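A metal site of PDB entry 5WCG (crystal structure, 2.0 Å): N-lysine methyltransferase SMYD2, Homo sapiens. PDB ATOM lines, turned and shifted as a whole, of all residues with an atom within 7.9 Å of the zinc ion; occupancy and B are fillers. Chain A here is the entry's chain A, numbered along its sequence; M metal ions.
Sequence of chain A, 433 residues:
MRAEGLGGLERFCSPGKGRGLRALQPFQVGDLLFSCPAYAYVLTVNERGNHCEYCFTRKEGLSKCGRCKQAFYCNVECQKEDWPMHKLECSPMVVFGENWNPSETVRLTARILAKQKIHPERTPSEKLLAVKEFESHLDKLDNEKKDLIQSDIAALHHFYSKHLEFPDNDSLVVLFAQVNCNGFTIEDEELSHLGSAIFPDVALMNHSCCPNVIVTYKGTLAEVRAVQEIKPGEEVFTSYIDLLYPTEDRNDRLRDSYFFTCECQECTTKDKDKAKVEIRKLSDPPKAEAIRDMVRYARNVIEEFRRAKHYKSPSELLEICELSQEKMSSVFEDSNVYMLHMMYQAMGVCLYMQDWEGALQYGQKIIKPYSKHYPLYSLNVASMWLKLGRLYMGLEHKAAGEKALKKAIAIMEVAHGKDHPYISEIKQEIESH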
ATOM      1  N   LYS A  64       8.837 -15.615 -25.039  1.00  0.00           N
ATOM      2  CA  LYS A  64       7.831 -15.806 -24.010  1.00  0.00           C
ATOM      3  C   LYS A  64       7.536 -17.280 -23.853  1.00  0.00           C
ATOM      4  O   LYS A  64       7.574 -18.010 -24.824  1.00  0.00           O
ATOM      5  CB  LYS A  64       6.581 -15.115 -24.532  1.00  0.00           C
ATOM      6  CG  LYS A  64       5.564 -14.742 -23.514  1.00  0.00           C
ATOM      7  CD  LYS A  64       4.443 -13.942 -24.175  1.00  0.00           C
ATOM      8  CE  LYS A  64       4.835 -12.489 -24.358  1.00  0.00           C
ATOM      9  NZ  LYS A  64       3.644 -11.629 -24.578  1.00  0.00           N
ATOM     10  N   CYS A  65       7.234 -17.728 -22.631  1.00  0.00           N
ATOM     11  CA  CYS A  65       6.625 -19.059 -22.438  1.00  0.00           C
ATOM     12  C   CYS A  65       5.219 -19.037 -23.025  1.00  0.00           C
ATOM     13  O   CYS A  65       4.362 -18.296 -22.574  1.00  0.00           O
ATOM     14  CB  CYS A  65       6.518 -19.426 -20.953  1.00  0.00           C
ATOM     15  SG  CYS A  65       5.672 -21.001 -20.707  1.00  0.00           S
ATOM     16  N   GLY A  66       4.962 -19.914 -23.994  1.00  0.00           N
ATOM     17  CA  GLY A  66       3.650 -19.948 -24.670  1.00  0.00           C
ATOM     18  C   GLY A  66       2.502 -20.397 -23.796  1.00  0.00           C
ATOM     19  O   GLY A  66       1.354 -20.078 -24.065  1.00  0.00           O
ATOM     20  N   ARG A  67       2.801 -21.130 -22.710  1.00  0.00           N
ATOM     21  CA  ARG A  67       1.752 -21.665 -21.854  1.00  0.00           C
ATOM     22  C   ARG A  67       1.207 -20.621 -20.915  1.00  0.00           C
ATOM     23  O   ARG A  67      -0.007 -20.466 -20.812  1.00  0.00           O
ATOM     24  CB  ARG A  67       2.293 -22.846 -21.066  1.00  0.00           C
ATOM     25  CG  ARG A  67       2.803 -23.963 -21.946  1.00  0.00           C
ATOM     26  CD  ARG A  67       3.669 -24.928 -21.166  1.00  0.00           C
ATOM     27  NE  ARG A  67       2.822 -25.737 -20.294  1.00  0.00           N
ATOM     28  CZ  ARG A  67       2.493 -27.020 -20.504  1.00  0.00           C
ATOM     29  NH1 ARG A  67       2.944 -27.687 -21.564  1.00  0.00           N
ATOM     30  NH2 ARG A  67       1.721 -27.655 -19.624  1.00  0.00           N
ATOM     31  N   CYS A  68       2.102 -19.930 -20.200  1.00  0.00           N
ATOM     32  CA  CYS A  68       1.663 -18.944 -19.196  1.00  0.00           C
ATOM     33  C   CYS A  68       1.832 -17.506 -19.637  1.00  0.00           C
ATOM     34  O   CYS A  68       1.192 -16.628 -19.065  1.00  0.00           O
ATOM     35  CB  CYS A  68       2.383 -19.160 -17.864  1.00  0.00           C
ATOM     36  SG  CYS A  68       4.164 -18.894 -17.887  1.00  0.00           S
ATOM     37  N   LYS A  69       2.701 -17.252 -20.611  1.00  0.00           N
ATOM     38  CA  LYS A  69       2.987 -15.890 -21.084  1.00  0.00           C
ATOM     39  C   LYS A  69       3.623 -14.974 -20.017  1.00  0.00           C
ATOM     40  O   LYS A  69       3.651 -13.763 -20.187  1.00  0.00           O
ATOM     41  CB  LYS A  69       1.718 -15.244 -21.697  1.00  0.00           C
ATOM     42  CG  LYS A  69       1.131 -16.104 -22.811  1.00  0.00           C
ATOM     43  CD  LYS A  69      -0.022 -15.424 -23.550  1.00  0.00           C
ATOM     44  CE  LYS A  69      -0.741 -16.437 -24.439  1.00  0.00           C
ATOM     45  NZ  LYS A  69       0.190 -17.117 -25.390  1.00  0.00           N
ATOM     46  N   GLN A  70       4.133 -15.548 -18.925  1.00  0.00           N
ATOM     47  CA  GLN A  70       4.681 -14.763 -17.819  1.00  0.00           C
ATOM     48  C   GLN A  70       6.128 -15.100 -17.490  1.00  0.00           C
ATOM     49  O   GLN A  70       6.652 -14.632 -16.481  1.00  0.00           O
ATOM     50  CB  GLN A  70       3.770 -14.878 -16.593  1.00  0.00           C
ATOM     51  CG  GLN A  70       2.411 -14.217 -16.813  1.00  0.00           C
ATOM     52  CD  GLN A  70       1.709 -13.822 -15.517  1.00  0.00           C
ATOM     53  OE1 GLN A  70       1.346 -14.674 -14.702  1.00  0.00           O
ATOM     54  NE2 GLN A  70       1.514 -12.530 -15.334  1.00  0.00           N
ATOM     55  N   ALA A  71       6.771 -15.907 -18.325  1.00  0.00           N
ATOM     56  CA  ALA A  71       8.203 -16.176 -18.157  1.00  0.00           C
ATOM     57  C   ALA A  71       8.915 -15.911 -19.490  1.00  0.00           C
ATOM     58  O   ALA A  71       8.438 -16.332 -20.550  1.00  0.00           O
ATOM     59  CB  ALA A  71       8.443 -17.606 -17.680  1.00  0.00           C
ATOM     60  N   PHE A  72      10.034 -15.205 -19.440  1.00  0.00           N
ATOM     61  CA  PHE A  72      10.796 -14.815 -20.644  1.00  0.00           C
ATOM     62  C   PHE A  72      12.213 -15.346 -20.591  1.00  0.00           C
ATOM     63  O   PHE A  72      12.793 -15.514 -19.486  1.00  0.00           O
ATOM     64  CB  PHE A  72      10.809 -13.304 -20.786  1.00  0.00           C
ATOM     65  CG  PHE A  72       9.444 -12.707 -20.926  1.00  0.00           C
ATOM     66  CD1 PHE A  72       8.600 -12.593 -19.812  1.00  0.00           C
ATOM     67  CD2 PHE A  72       8.995 -12.252 -22.163  1.00  0.00           C
ATOM     68  CE1 PHE A  72       7.315 -12.053 -19.949  1.00  0.00           C
ATOM     69  CE2 PHE A  72       7.733 -11.689 -22.287  1.00  0.00           C
ATOM     70  CZ  PHE A  72       6.899 -11.595 -21.185  1.00  0.00           C
ATOM     71  N   TYR A  73      12.766 -15.594 -21.786  1.00  0.00           N
ATOM     72  CA  TYR A  73      14.013 -16.340 -21.984  1.00  0.00           C
ATOM     73  C   TYR A  73      14.830 -15.790 -23.158  1.00  0.00           C
ATOM     74  O   TYR A  73      14.264 -15.236 -24.100  1.00  0.00           O
ATOM     75  CB  TYR A  73      13.694 -17.808 -22.252  1.00  0.00           C
ATOM     76  CG  TYR A  73      12.974 -18.480 -21.084  1.00  0.00           C
ATOM     77  CD1 TYR A  73      13.668 -18.769 -19.926  1.00  0.00           C
ATOM     78  CD2 TYR A  73      11.620 -18.791 -21.148  1.00  0.00           C
ATOM     79  CE1 TYR A  73      13.034 -19.377 -18.856  1.00  0.00           C
ATOM     80  CE2 TYR A  73      10.973 -19.399 -20.071  1.00  0.00           C
ATOM     81  CZ  TYR A  73      11.689 -19.690 -18.917  1.00  0.00           C
ATOM     82  OH  TYR A  73      11.092 -20.308 -17.837  1.00  0.00           O
ATOM     83  N   GLN A  79      14.980 -21.553 -21.989  1.00  0.00           N
ATOM     84  CA  GLN A  79      13.628 -21.934 -21.648  1.00  0.00           C
ATOM     85  C   GLN A  79      13.543 -23.385 -21.216  1.00  0.00           C
ATOM     86  O   GLN A  79      12.919 -23.684 -20.205  1.00  0.00           O
ATOM     87  CB  GLN A  79      12.660 -21.685 -22.818  1.00  0.00           C
ATOM     88  CG  GLN A  79      11.252 -22.226 -22.584  1.00  0.00           C
ATOM     89  CD  GLN A  79      10.258 -21.886 -23.688  1.00  0.00           C
ATOM     90  OE1 GLN A  79       9.032 -21.916 -23.478  1.00  0.00           O
ATOM     91  NE2 GLN A  79      10.768 -21.567 -24.850  1.00  0.00           N
ATOM     92  N   TRP A  83      12.882 -25.178 -17.310  1.00  0.00           N
ATOM     93  CA  TRP A  83      11.565 -25.861 -17.195  1.00  0.00           C
ATOM     94  C   TRP A  83      11.321 -26.625 -15.861  1.00  0.00           C
ATOM     95  O   TRP A  83      10.242 -26.514 -15.306  1.00  0.00           O
ATOM     96  CB  TRP A  83      11.249 -26.706 -18.432  1.00  0.00           C
ATOM     97  CG  TRP A  83       9.943 -27.465 -18.351  1.00  0.00           C
ATOM     98  CD1 TRP A  83       9.779 -28.830 -18.258  1.00  0.00           C
ATOM     99  CD2 TRP A  83       8.627 -26.905 -18.312  1.00  0.00           C
ATOM    100  NE1 TRP A  83       8.439 -29.141 -18.177  1.00  0.00           N
ATOM    101  CE2 TRP A  83       7.714 -27.985 -18.216  1.00  0.00           C
ATOM    102  CE3 TRP A  83       8.135 -25.600 -18.361  1.00  0.00           C
ATOM    103  CZ2 TRP A  83       6.340 -27.789 -18.155  1.00  0.00           C
ATOM    104  CZ3 TRP A  83       6.782 -25.399 -18.293  1.00  0.00           C
ATOM    105  CH2 TRP A  83       5.892 -26.489 -18.213  1.00  0.00           C
ATOM    106  N   HIS A  86      10.518 -23.677 -13.545  1.00  0.00           N
ATOM    107  CA  HIS A  86       9.356 -22.929 -14.027  1.00  0.00           C
ATOM    108  C   HIS A  86       8.026 -23.713 -13.958  1.00  0.00           C
ATOM    109  O   HIS A  86       6.981 -23.124 -13.707  1.00  0.00           O
ATOM    110  CB  HIS A  86       9.587 -22.425 -15.442  1.00  0.00           C
ATOM    111  CG  HIS A  86       8.421 -21.721 -16.030  1.00  0.00           C
ATOM    112  ND1 HIS A  86       7.885 -20.583 -15.476  1.00  0.00           N
ATOM    113  CD2 HIS A  86       7.674 -21.995 -17.134  1.00  0.00           C
ATOM    114  CE1 HIS A  86       6.860 -20.183 -16.202  1.00  0.00           C
ATOM    115  NE2 HIS A  86       6.726 -21.014 -17.228  1.00  0.00           N
ATOM    116  N   LYS A  87       8.065 -25.021 -14.131  1.00  0.00           N
ATOM    117  CA  LYS A  87       6.850 -25.822 -14.115  1.00  0.00           C
ATOM    118  C   LYS A  87       6.154 -25.860 -12.739  1.00  0.00           C
ATOM    119  O   LYS A  87       4.974 -26.204 -12.646  1.00  0.00           O
ATOM    120  CB  LYS A  87       7.122 -27.255 -14.604  1.00  0.00           C
ATOM    121  CG  LYS A  87       7.805 -28.145 -13.589  1.00  0.00           C
ATOM    122  CD  LYS A  87       7.567 -29.611 -13.959  1.00  0.00           C
ATOM    123  CE  LYS A  87       8.691 -30.517 -13.491  1.00  0.00           C
ATOM    124  NZ  LYS A  87       8.701 -31.737 -14.351  1.00  0.00           N
ATOM    125  N   GLU A  89       5.477 -23.151 -11.291  1.00  0.00           N
ATOM    126  CA  GLU A  89       4.627 -21.965 -11.353  1.00  0.00           C
ATOM    127  C   GLU A  89       3.801 -21.793 -12.611  1.00  0.00           C
ATOM    128  O   GLU A  89       2.850 -21.041 -12.595  1.00  0.00           O
ATOM    129  CB  GLU A  89       5.509 -20.699 -11.151  1.00  0.00           C
ATOM    130  CG  GLU A  89       6.239 -20.756  -9.823  1.00  0.00           C
ATOM    131  CD  GLU A  89       7.121 -19.575  -9.543  1.00  0.00           C
ATOM    132  OE1 GLU A  89       7.694 -18.990 -10.487  1.00  0.00           O
ATOM    133  OE2 GLU A  89       7.249 -19.252  -8.349  1.00  0.00           O
ATOM    134  N   CYS A  90       4.130 -22.496 -13.686  1.00  0.00           N
ATOM    135  CA  CYS A  90       3.541 -22.197 -14.991  1.00  0.00           C
ATOM    136  C   CYS A  90       1.997 -22.395 -14.952  1.00  0.00           C
ATOM    137  O   CYS A  90       1.228 -21.441 -15.144  1.00  0.00           O
ATOM    138  CB  CYS A  90       4.222 -23.036 -16.078  1.00  0.00           C
ATOM    139  SG  CYS A  90       3.638 -22.705 -17.771  1.00  0.00           S
ATOM    140  N   SER A  91       1.556 -23.628 -14.694  1.00  0.00           N
ATOM    141  CA  SER A  91       0.112 -23.880 -14.602  1.00  0.00           C
ATOM    142  C   SER A  91      -0.560 -23.103 -13.450  1.00  0.00           C
ATOM    143  O   SER A  91      -1.650 -22.556 -13.630  1.00  0.00           O
ATOM    144  CB  SER A  91      -0.190 -25.382 -14.529  1.00  0.00           C
ATOM    145  OG  SER A  91      -1.574 -25.597 -14.345  1.00  0.00           O
ATOM    146  N   MET A  93       0.060 -20.108 -12.306  1.00  0.00           N
ATOM    147  CA  MET A  93      -0.175 -18.760 -12.800  1.00  0.00           C
ATOM    148  C   MET A  93      -1.373 -18.660 -13.732  1.00  0.00           C
ATOM    149  O   MET A  93      -2.072 -17.672 -13.713  1.00  0.00           O
ATOM    150  CB  MET A  93       1.069 -18.185 -13.509  1.00  0.00           C
ATOM    151  CG  MET A  93       2.167 -17.795 -12.524  1.00  0.00           C
ATOM    152  SD  MET A  93       3.529 -16.859 -13.246  1.00  0.00           S
ATOM    153  CE  MET A  93       4.363 -18.113 -14.191  1.00  0.00           C
ATOM    154  N   VAL A  94      -1.589 -19.697 -14.529  1.00  0.00           N
ATOM    155  CA  VAL A  94      -2.724 -19.785 -15.438  1.00  0.00           C
ATOM    156  C   VAL A  94      -3.981 -20.025 -14.597  1.00  0.00           C
ATOM    157  O   VAL A  94      -4.971 -19.322 -14.722  1.00  0.00           O
ATOM    158  CB  VAL A  94      -2.541 -20.925 -16.472  1.00  0.00           C
ATOM    159  CG1 VAL A  94      -3.782 -21.114 -17.363  1.00  0.00           C
ATOM    160  CG2 VAL A  94      -1.319 -20.690 -17.347  1.00  0.00           C
HETATM  161 ZN    ZN M   1       4.985 -20.866 -18.357  1.00  0.00          ZN
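N of Gln 70 lies close to SG of Cys 68 (3.5 Å).
The backbone NH (N) of Arg 67 lies close to the side-chain sulfur (SG) of Cys 65 (3.5 Å).
N of Cys 65 lies within hydrogen-bond range of O of Ala 71 (2.8 Å).
Of the 19 residues printed, 4 come within 4 Å of the zinc ion.
The nearest printed residue that does not touch the zinc ion is Arg 67 (4.3 Å).
The zinc ion is bound by NE2 of His 86 (2.1 Å).
The zinc ion is bound by the side-chain sulfur (SG) of Cys 68 (2.2 Å).
SG of Cys 90 is bound to the zinc ion (2.4 Å).
The side-chain sulfur (SG) of Cys 65 binds the zinc ion (2.5 Å).
The zinc ion has four donor atoms within binding distance.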
